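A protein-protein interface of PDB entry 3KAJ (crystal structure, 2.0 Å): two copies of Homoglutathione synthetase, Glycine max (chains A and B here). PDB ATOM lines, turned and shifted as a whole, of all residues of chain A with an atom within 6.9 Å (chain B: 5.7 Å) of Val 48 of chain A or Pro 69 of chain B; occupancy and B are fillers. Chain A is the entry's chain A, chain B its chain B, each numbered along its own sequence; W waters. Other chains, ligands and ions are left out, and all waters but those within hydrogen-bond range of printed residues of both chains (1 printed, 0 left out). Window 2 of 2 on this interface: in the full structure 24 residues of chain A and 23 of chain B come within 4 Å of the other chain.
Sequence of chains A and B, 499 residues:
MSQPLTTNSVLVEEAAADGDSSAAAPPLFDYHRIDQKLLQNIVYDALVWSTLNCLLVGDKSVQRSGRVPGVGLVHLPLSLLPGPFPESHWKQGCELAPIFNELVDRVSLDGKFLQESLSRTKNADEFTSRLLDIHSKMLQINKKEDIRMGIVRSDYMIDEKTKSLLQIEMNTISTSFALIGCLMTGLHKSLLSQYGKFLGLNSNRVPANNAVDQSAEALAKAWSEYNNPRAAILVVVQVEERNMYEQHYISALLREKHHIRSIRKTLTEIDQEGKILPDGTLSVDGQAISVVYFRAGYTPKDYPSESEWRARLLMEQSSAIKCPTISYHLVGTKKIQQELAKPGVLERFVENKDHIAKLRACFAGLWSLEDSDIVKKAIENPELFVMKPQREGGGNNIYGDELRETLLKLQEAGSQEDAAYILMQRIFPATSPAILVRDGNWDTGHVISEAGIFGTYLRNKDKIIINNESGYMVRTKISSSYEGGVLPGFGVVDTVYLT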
ATOM      1  N   GLN A  40       7.503 -23.239  11.316  1.00  0.00           N
ATOM      2  CA  GLN A  40       8.109 -24.322  10.528  1.00  0.00           C
ATOM      3  C   GLN A  40       7.084 -25.448  10.333  1.00  0.00           C
ATOM      4  O   GLN A  40       6.950 -25.966   9.239  1.00  0.00           O
ATOM      5  CB  GLN A  40       9.387 -24.827  11.186  1.00  0.00           C
ATOM      6  CG  GLN A  40      10.110 -25.955  10.475  1.00  0.00           C
ATOM      7  CD  GLN A  40      10.479 -25.602   9.052  1.00  0.00           C
ATOM      8  OE1 GLN A  40      10.796 -24.451   8.752  1.00  0.00           O
ATOM      9  NE2 GLN A  40      10.446 -26.601   8.167  1.00  0.00           N
ATOM     10  N   VAL A  43       4.456 -24.393   7.772  1.00  0.00           N
ATOM     11  CA  VAL A  43       5.091 -24.358   6.457  1.00  0.00           C
ATOM     12  C   VAL A  43       5.283 -25.776   5.921  1.00  0.00           C
ATOM     13  O   VAL A  43       5.026 -26.061   4.738  1.00  0.00           O
ATOM     14  CB  VAL A  43       6.446 -23.683   6.519  1.00  0.00           C
ATOM     15  CG1 VAL A  43       7.240 -23.964   5.139  1.00  0.00           C
ATOM     16  CG2 VAL A  43       6.253 -22.222   6.698  1.00  0.00           C
ATOM     17  N   TYR A  44       5.719 -26.670   6.778  1.00  0.00           N
ATOM     18  CA  TYR A  44       5.886 -28.053   6.340  1.00  0.00           C
ATOM     19  C   TYR A  44       4.543 -28.611   5.865  1.00  0.00           C
ATOM     20  O   TYR A  44       4.477 -29.212   4.811  1.00  0.00           O
ATOM     21  CB  TYR A  44       6.527 -28.871   7.442  1.00  0.00           C
ATOM     22  CG  TYR A  44       6.797 -30.320   7.043  1.00  0.00           C
ATOM     23  CD1 TYR A  44       8.050 -30.718   6.635  1.00  0.00           C
ATOM     24  CD2 TYR A  44       5.789 -31.261   7.072  1.00  0.00           C
ATOM     25  CE1 TYR A  44       8.315 -32.058   6.298  1.00  0.00           C
ATOM     26  CE2 TYR A  44       6.044 -32.592   6.724  1.00  0.00           C
ATOM     27  CZ  TYR A  44       7.298 -32.978   6.313  1.00  0.00           C
ATOM     28  OH  TYR A  44       7.568 -34.317   5.969  1.00  0.00           O
ATOM     29  N   ASP A  45       3.440 -28.327   6.580  1.00  0.00           N
ATOM     30  CA  ASP A  45       2.125 -28.843   6.204  1.00  0.00           C
ATOM     31  C   ASP A  45       1.694 -28.225   4.875  1.00  0.00           C
ATOM     32  O   ASP A  45       1.027 -28.875   4.101  1.00  0.00           O
ATOM     33  CB  ASP A  45       1.060 -28.535   7.305  1.00  0.00           C
ATOM     34  CG  ASP A  45       1.196 -29.431   8.515  1.00  0.00           C
ATOM     35  OD1 ASP A  45       1.974 -30.407   8.411  1.00  0.00           O
ATOM     36  OD2 ASP A  45       0.603 -29.182   9.590  1.00  0.00           O
ATOM     37  N   ALA A  46       2.086 -26.971   4.617  1.00  0.00           N
ATOM     38  CA  ALA A  46       1.713 -26.309   3.370  1.00  0.00           C
ATOM     39  C   ALA A  46       2.406 -26.899   2.173  1.00  0.00           C
ATOM     40  O   ALA A  46       1.787 -27.017   1.055  1.00  0.00           O
ATOM     41  CB  ALA A  46       1.990 -24.796   3.459  1.00  0.00           C
ATOM     42  N   LEU A  47       3.690 -27.262   2.370  1.00  0.00           N
ATOM     43  CA  LEU A  47       4.533 -27.784   1.285  1.00  0.00           C
ATOM     44  C   LEU A  47       4.009 -29.167   0.927  1.00  0.00           C
ATOM     45  O   LEU A  47       3.972 -29.535  -0.246  1.00  0.00           O
ATOM     46  CB  LEU A  47       5.980 -27.881   1.730  1.00  0.00           C
ATOM     47  CG  LEU A  47       6.691 -26.533   1.893  1.00  0.00           C
ATOM     48  CD1 LEU A  47       8.075 -26.655   2.593  1.00  0.00           C
ATOM     49  CD2 LEU A  47       6.821 -25.833   0.568  1.00  0.00           C
ATOM     50  N   VAL A  48       3.651 -29.918   1.962  1.00  0.00           N
ATOM     51  CA  VAL A  48       2.960 -31.253   1.826  1.00  0.00           C
ATOM     52  C   VAL A  48       1.671 -31.077   1.010  1.00  0.00           C
ATOM     53  O   VAL A  48       1.513 -31.741  -0.036  1.00  0.00           O
ATOM     54  CB  VAL A  48       2.708 -31.927   3.199  1.00  0.00           C
ATOM     55  CG1 VAL A  48       1.567 -33.060   3.144  1.00  0.00           C
ATOM     56  CG2 VAL A  48       4.027 -32.483   3.816  1.00  0.00           C
ATOM     57  N   TRP A  49       0.767 -30.174   1.453  1.00  0.00           N
ATOM     58  CA  TRP A  49      -0.589 -29.993   0.840  1.00  0.00           C
ATOM     59  C   TRP A  49      -0.442 -29.539  -0.593  1.00  0.00           C
ATOM     60  O   TRP A  49      -1.118 -30.046  -1.538  1.00  0.00           O
ATOM     61  CB  TRP A  49      -1.400 -28.902   1.595  1.00  0.00           C
ATOM     62  CG  TRP A  49      -2.899 -28.873   1.214  1.00  0.00           C
ATOM     63  CD1 TRP A  49      -3.924 -29.458   1.927  1.00  0.00           C
ATOM     64  CD2 TRP A  49      -3.521 -28.238   0.087  1.00  0.00           C
ATOM     65  NE1 TRP A  49      -5.126 -29.212   1.336  1.00  0.00           N
ATOM     66  CE2 TRP A  49      -4.915 -28.502   0.181  1.00  0.00           C
ATOM     67  CE3 TRP A  49      -3.046 -27.492  -1.015  1.00  0.00           C
ATOM     68  CZ2 TRP A  49      -5.802 -28.069  -0.767  1.00  0.00           C
ATOM     69  CZ3 TRP A  49      -3.964 -27.060  -1.987  1.00  0.00           C
ATOM     70  CH2 TRP A  49      -5.310 -27.322  -1.841  1.00  0.00           C
ATOM     71  N   SER A  50       0.498 -28.620  -0.790  1.00  0.00           N
ATOM     72  CA  SER A  50       0.811 -28.140  -2.154  1.00  0.00           C
ATOM     73  C   SER A  50       1.164 -29.241  -3.159  1.00  0.00           C
ATOM     74  O   SER A  50       0.700 -29.201  -4.330  1.00  0.00           O
ATOM     75  CB  SER A  50       1.942 -27.102  -2.091  1.00  0.00           C
ATOM     76  OG  SER A  50       1.477 -25.877  -1.450  1.00  0.00           O
ATOM     77  N   THR A  51       2.001 -30.195  -2.728  1.00  0.00           N
ATOM     78  CA  THR A  51       2.452 -31.321  -3.617  1.00  0.00           C
ATOM     79  C   THR A  51       1.262 -32.294  -3.880  1.00  0.00           C
ATOM     80  O   THR A  51       1.014 -32.710  -5.000  1.00  0.00           O
ATOM     81  CB  THR A  51       3.659 -32.071  -3.013  1.00  0.00           C
ATOM     82  OG1 THR A  51       4.625 -31.117  -2.511  1.00  0.00           O
ATOM     83  CG2 THR A  51       4.324 -32.983  -4.071  1.00  0.00           C
ATOM     84  N   LEU A  52       0.512 -32.622  -2.834  1.00  0.00           N
ATOM     85  CA  LEU A  52      -0.592 -33.583  -2.952  1.00  0.00           C
ATOM     86  C   LEU A  52      -1.705 -33.057  -3.838  1.00  0.00           C
ATOM     87  O   LEU A  52      -2.385 -33.828  -4.499  1.00  0.00           O
ATOM     88  CB  LEU A  52      -1.155 -33.942  -1.577  1.00  0.00           C
ATOM     89  CG  LEU A  52      -0.274 -34.805  -0.673  1.00  0.00           C
ATOM     90  CD1 LEU A  52      -1.015 -34.949   0.651  1.00  0.00           C
ATOM     91  CD2 LEU A  52       0.069 -36.204  -1.275  1.00  0.00           C
ATOM     92  N   ASN A  53      -1.863 -31.728  -3.872  1.00  0.00           N
ATOM     93  CA  ASN A  53      -2.953 -31.117  -4.629  1.00  0.00           C
ATOM     94  C   ASN A  53      -2.546 -30.294  -5.851  1.00  0.00           C
ATOM     95  O   ASN A  53      -3.367 -29.528  -6.354  1.00  0.00           O
ATOM     96  CB  ASN A  53      -3.805 -30.298  -3.657  1.00  0.00           C
ATOM     97  CG  ASN A  53      -4.467 -31.166  -2.647  1.00  0.00           C
ATOM     98  OD1 ASN A  53      -5.496 -31.751  -2.935  1.00  0.00           O
ATOM     99  ND2 ASN A  53      -3.891 -31.264  -1.452  1.00  0.00           N
ATOM    100  N   HIS A  75       6.682 -26.213  -5.581  1.00  0.00           N
ATOM    101  CA  HIS A  75       5.433 -25.638  -5.128  1.00  0.00           C
ATOM    102  C   HIS A  75       5.421 -24.192  -5.598  1.00  0.00           C
ATOM    103  O   HIS A  75       6.477 -23.627  -5.858  1.00  0.00           O
ATOM    104  CB  HIS A  75       5.379 -25.708  -3.599  1.00  0.00           C
ATOM    105  CG  HIS A  75       6.307 -24.749  -2.922  1.00  0.00           C
ATOM    106  ND1 HIS A  75       5.927 -23.471  -2.557  1.00  0.00           N
ATOM    107  CD2 HIS A  75       7.612 -24.873  -2.578  1.00  0.00           C
ATOM    108  CE1 HIS A  75       6.982 -22.843  -2.037  1.00  0.00           C
ATOM    109  NE2 HIS A  75       8.003 -23.685  -2.012  1.00  0.00           N
ATOM    110  N   LEU A 187      -5.747 -24.626   0.415  1.00  0.00           N
ATOM    111  CA  LEU A 187      -4.655 -24.649   1.318  1.00  0.00           C
ATOM    112  C   LEU A 187      -4.906 -23.865   2.591  1.00  0.00           C
ATOM    113  O   LEU A 187      -4.719 -24.402   3.699  1.00  0.00           O
ATOM    114  CB  LEU A 187      -3.409 -24.103   0.654  1.00  0.00           C
ATOM    115  CG  LEU A 187      -2.302 -24.078   1.686  1.00  0.00           C
ATOM    116  CD1 LEU A 187      -1.797 -25.489   2.031  1.00  0.00           C
ATOM    117  CD2 LEU A 187      -1.203 -23.225   1.046  1.00  0.00           C
ATOM    118  N   ASP A 439      10.670 -21.826  -2.896  1.00  0.00           N
ATOM    119  CA  ASP A 439      11.620 -22.980  -3.068  1.00  0.00           C
ATOM    120  C   ASP A 439      11.946 -23.718  -1.724  1.00  0.00           C
ATOM    121  O   ASP A 439      13.089 -23.996  -1.392  1.00  0.00           O
ATOM    122  CB  ASP A 439      12.851 -22.469  -3.851  1.00  0.00           C
ATOM    123  CG  ASP A 439      13.884 -23.517  -4.081  1.00  0.00           C
ATOM    124  OD1 ASP A 439      15.091 -23.167  -3.885  1.00  0.00           O
ATOM    125  OD2 ASP A 439      13.510 -24.670  -4.469  1.00  0.00           O
ATOM    126  N   GLY A 440      10.911 -23.951  -0.919  1.00  0.00           N
ATOM    127  CA  GLY A 440      10.979 -24.764   0.295  1.00  0.00           C
ATOM    128  C   GLY A 440      11.370 -24.018   1.569  1.00  0.00           C
ATOM    129  O   GLY A 440      11.413 -24.583   2.606  1.00  0.00           O
ATOM    130  N   ARG B  64      17.750 -32.004  -1.376  1.00  0.00           N
ATOM    131  CA  ARG B  64      16.785 -31.788  -0.308  1.00  0.00           C
ATOM    132  C   ARG B  64      15.455 -32.536  -0.495  1.00  0.00           C
ATOM    133  O   ARG B  64      14.605 -32.465   0.374  1.00  0.00           O
ATOM    134  CB  ARG B  64      16.410 -30.317  -0.220  1.00  0.00           C
ATOM    135  CG  ARG B  64      17.489 -29.361   0.225  1.00  0.00           C
ATOM    136  CD  ARG B  64      17.277 -28.065  -0.569  1.00  0.00           C
ATOM    137  NE  ARG B  64      16.220 -27.265   0.023  1.00  0.00           N
ATOM    138  CZ  ARG B  64      15.416 -26.411  -0.624  1.00  0.00           C
ATOM    139  NH1 ARG B  64      15.479 -26.214  -1.933  1.00  0.00           N
ATOM    140  NH2 ARG B  64      14.521 -25.776   0.080  1.00  0.00           N
ATOM    141  N   ARG B  67      13.703 -34.721   2.158  1.00  0.00           N
ATOM    142  CA  ARG B  67      13.504 -34.071   3.431  1.00  0.00           C
ATOM    143  C   ARG B  67      12.533 -32.866   3.392  1.00  0.00           C
ATOM    144  O   ARG B  67      11.796 -32.591   4.355  1.00  0.00           O
ATOM    145  CB  ARG B  67      14.863 -33.552   3.920  1.00  0.00           C
ATOM    146  CG  ARG B  67      15.751 -34.618   4.469  1.00  0.00           C
ATOM    147  CD  ARG B  67      17.052 -33.997   4.976  1.00  0.00           C
ATOM    148  NE  ARG B  67      17.995 -33.911   3.867  1.00  0.00           N
ATOM    149  CZ  ARG B  67      18.404 -32.777   3.300  1.00  0.00           C
ATOM    150  NH1 ARG B  67      17.997 -31.599   3.760  1.00  0.00           N
ATOM    151  NH2 ARG B  67      19.248 -32.828   2.286  1.00  0.00           N
ATOM    152  N   VAL B  68      12.587 -32.098   2.327  1.00  0.00           N
ATOM    153  CA  VAL B  68      11.713 -30.887   2.263  1.00  0.00           C
ATOM    154  C   VAL B  68      10.556 -31.149   1.274  1.00  0.00           C
ATOM    155  O   VAL B  68      10.797 -31.267   0.084  1.00  0.00           O
ATOM    156  CB  VAL B  68      12.565 -29.633   1.805  1.00  0.00           C
ATOM    157  CG1 VAL B  68      11.696 -28.349   1.719  1.00  0.00           C
ATOM    158  CG2 VAL B  68      13.826 -29.467   2.736  1.00  0.00           C
ATOM    159  N   PRO B  69       9.300 -31.137   1.740  1.00  0.00           N
ATOM    160  CA  PRO B  69       8.211 -31.320   0.759  1.00  0.00           C
ATOM    161  C   PRO B  69       8.144 -30.165  -0.255  1.00  0.00           C
ATOM    162  O   PRO B  69       8.547 -29.035   0.051  1.00  0.00           O
ATOM    163  CB  PRO B  69       6.930 -31.343   1.626  1.00  0.00           C
ATOM    164  CG  PRO B  69       7.441 -31.569   3.052  1.00  0.00           C
ATOM    165  CD  PRO B  69       8.787 -30.896   3.103  1.00  0.00           C
ATOM    166  N   GLY B  70       7.649 -30.434  -1.455  1.00  0.00           N
ATOM    167  CA  GLY B  70       7.297 -29.332  -2.331  1.00  0.00           C
ATOM    168  C   GLY B  70       8.433 -28.943  -3.235  1.00  0.00           C
ATOM    169  O   GLY B  70       8.254 -28.055  -4.054  1.00  0.00           O
ATOM    170  N   VAL B  71       9.618 -29.544  -3.059  1.00  0.00           N
ATOM    171  CA  VAL B  71      10.803 -29.203  -3.833  1.00  0.00           C
ATOM    172  C   VAL B  71      11.422 -30.409  -4.551  1.00  0.00           C
ATOM    173  O   VAL B  71      11.269 -31.570  -4.117  1.00  0.00           O
ATOM    174  CB  VAL B  71      11.887 -28.448  -2.987  1.00  0.00           C
ATOM    175  CG1 VAL B  71      11.261 -27.296  -2.198  1.00  0.00           C
ATOM    176  CG2 VAL B  71      12.638 -29.366  -2.079  1.00  0.00           C
ATOM    177  N   MET B 244       7.721 -39.549   0.295  1.00  0.00           N
ATOM    178  CA  MET B 244       6.946 -39.110   1.480  1.00  0.00           C
ATOM    179  C   MET B 244       5.475 -38.820   1.174  1.00  0.00           C
ATOM    180  O   MET B 244       4.586 -38.972   2.033  1.00  0.00           O
ATOM    181  CB  MET B 244       7.572 -37.848   2.085  1.00  0.00           C
ATOM    182  CG  MET B 244       7.731 -36.724   1.062  1.00  0.00           C
ATOM    183  SD  MET B 244       8.159 -35.185   1.870  1.00  0.00           S
ATOM    184  CE  MET B 244       9.913 -35.231   1.537  1.00  0.00           C
ATOM    185  N   TYR B 245       5.192 -38.462  -0.061  1.00  0.00           N
ATOM    186  CA  TYR B 245       3.827 -38.115  -0.421  1.00  0.00           C
ATOM    187  C   TYR B 245       2.804 -39.234  -0.305  1.00  0.00           C
ATOM    188  O   TYR B 245       1.691 -38.959   0.095  1.00  0.00           O
ATOM    189  CB  TYR B 245       3.812 -37.383  -1.763  1.00  0.00           C
ATOM    190  CG  TYR B 245       4.866 -36.298  -1.722  1.00  0.00           C
ATOM    191  CD1 TYR B 245       6.099 -36.502  -2.321  1.00  0.00           C
ATOM    192  CD2 TYR B 245       4.640 -35.115  -1.055  1.00  0.00           C
ATOM    193  CE1 TYR B 245       7.096 -35.569  -2.237  1.00  0.00           C
ATOM    194  CE2 TYR B 245       5.635 -34.134  -0.999  1.00  0.00           C
ATOM    195  CZ  TYR B 245       6.852 -34.382  -1.621  1.00  0.00           C
ATOM    196  OH  TYR B 245       7.852 -33.489  -1.617  1.00  0.00           O
ATOM    197  N   HIS B 248       2.121 -39.028   3.273  1.00  0.00           N
ATOM    198  CA  HIS B 248       1.350 -37.832   3.536  1.00  0.00           C
ATOM    199  C   HIS B 248      -0.118 -38.010   3.132  1.00  0.00           C
ATOM    200  O   HIS B 248      -1.024 -37.559   3.876  1.00  0.00           O
ATOM    201  CB  HIS B 248       1.951 -36.607   2.888  1.00  0.00           C
ATOM    202  CG  HIS B 248       3.259 -36.205   3.508  1.00  0.00           C
ATOM    203  ND1 HIS B 248       3.381 -35.916   4.852  1.00  0.00           N
ATOM    204  CD2 HIS B 248       4.471 -35.981   2.958  1.00  0.00           C
ATOM    205  CE1 HIS B 248       4.641 -35.605   5.116  1.00  0.00           C
ATOM    206  NE2 HIS B 248       5.316 -35.590   3.974  1.00  0.00           N
HETATM  207  O   HOH W   1      10.081 -34.626   5.628  1.00  0.00           O
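Of the 16 printed residues of chain A, 8 touch a printed residue of chain B.
Of the 9 printed residues of chain B, 7 touch a printed residue of chain A.
Printed residues of chain B that touch a printed residue of chain A: Arg 64, Val 68, Pro 69, Gly 70, Val 71, Tyr 245 and His 248.
Hydrophobic or aromatic side chains of chain B that line the printed part of chain A: Val 68, Pro 69, Val 71, Tyr 245 and His 248.
Among the printed residues, Asp or Glu carboxylates within 4 Å of a Lys or Arg side-chain nitrogen of the other chain: Asp 439 of chain A with Arg 64 of chain B.
The guanidinium group (NH1) of Arg 64 of chain B is in salt-bridge range of the side-chain carboxylate (OD2) of Asp 439 of chain A, at 3.6 Å.
N of Gly 70 of chain B sits close to OG1 of Thr 51 of chain A, at 3.3 Å.
O of Gly 70 of chain B sits at hydrogen-bond distance from N of His 75 of chain A (2.9 Å).
A ring nitrogen (NE2) of His 248 of chain B is in hydrogen-bond range of the side-chain hydroxyl (OH) of Tyr 44 of chain A, at 3.3 Å.
Among the printed residues, merely in contact across the chains: Leu 47 of chain A with Pro 69 of chain B, Val 48 of chain A with His 248 of chain B, Tyr 44 of chain A with Pro 69 of chain B, Leu 52 of chain A with Tyr 245 of chain B, Thr 51 of chain A with Tyr 245 of chain B, Gly 440 of chain A with Val 71 of chain B, Val 48 of chain A with Pro 69 of chain B, Asp 439 of chain A with Val 71 of chain B, Gly 440 of chain A with Arg 64 of chain B, Gly 440 of chain A with Val 68 of chain B and Leu 47 of chain A with Gly 70 of chain B.
Printed residues of chain B within 4 Å of Tyr 44 of chain A: Pro 69 (3.4 Å) and His 248 (3.3 Å).
Val 48 of chain A touches just these residues of chain B: Pro 69 and His 248.
Printed residues of chain B within 4 Å of Gly 440 of chain A: Arg 64 (3.7 Å), Val 68 (3.9 Å) and Val 71 (3.6 Å).
Of chain A, only Tyr 44, Leu 47 and Val 48 come within 4 Å of Pro 69 of chain B.
The nearest printed residue of chain B that does not touch Gly 440 of chain A is Pro 69 of chain B (4.9 Å).
No position is printed for both chains.
Of the 15 pairs that touch across the chains among the printed residues, none has its exchanged pair printed and touching as well.
Water W1 bridges OH of Tyr 44 of chain A and O of Arg 67 of chain B.
The backbone carbonyl oxygen (O) of Leu 47 of chain A sits at hydrogen-bond distance from the side-chain hydroxyl (OG1) of Thr 51 of chain A, 2.8 Å away.
The backbone NH of Gly 70 of chain B is in hydrogen-bond range of the side-chain hydroxyl of Tyr 245 of chain B (3.1 Å).
A ring nitrogen (NE2) of His 75 of chain A lies within hydrogen-bond range of the backbone NH (N) of Gly 440 of chain A, at 3.1 Å.
NE2 of His 75 of chain A sits at hydrogen-bond distance from N of Asp 439 of chain A (3.4 Å).
NE2 of His 248 of chain B lies within hydrogen-bond range of SD of Met 244 of chain B, 3.6 Å away.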
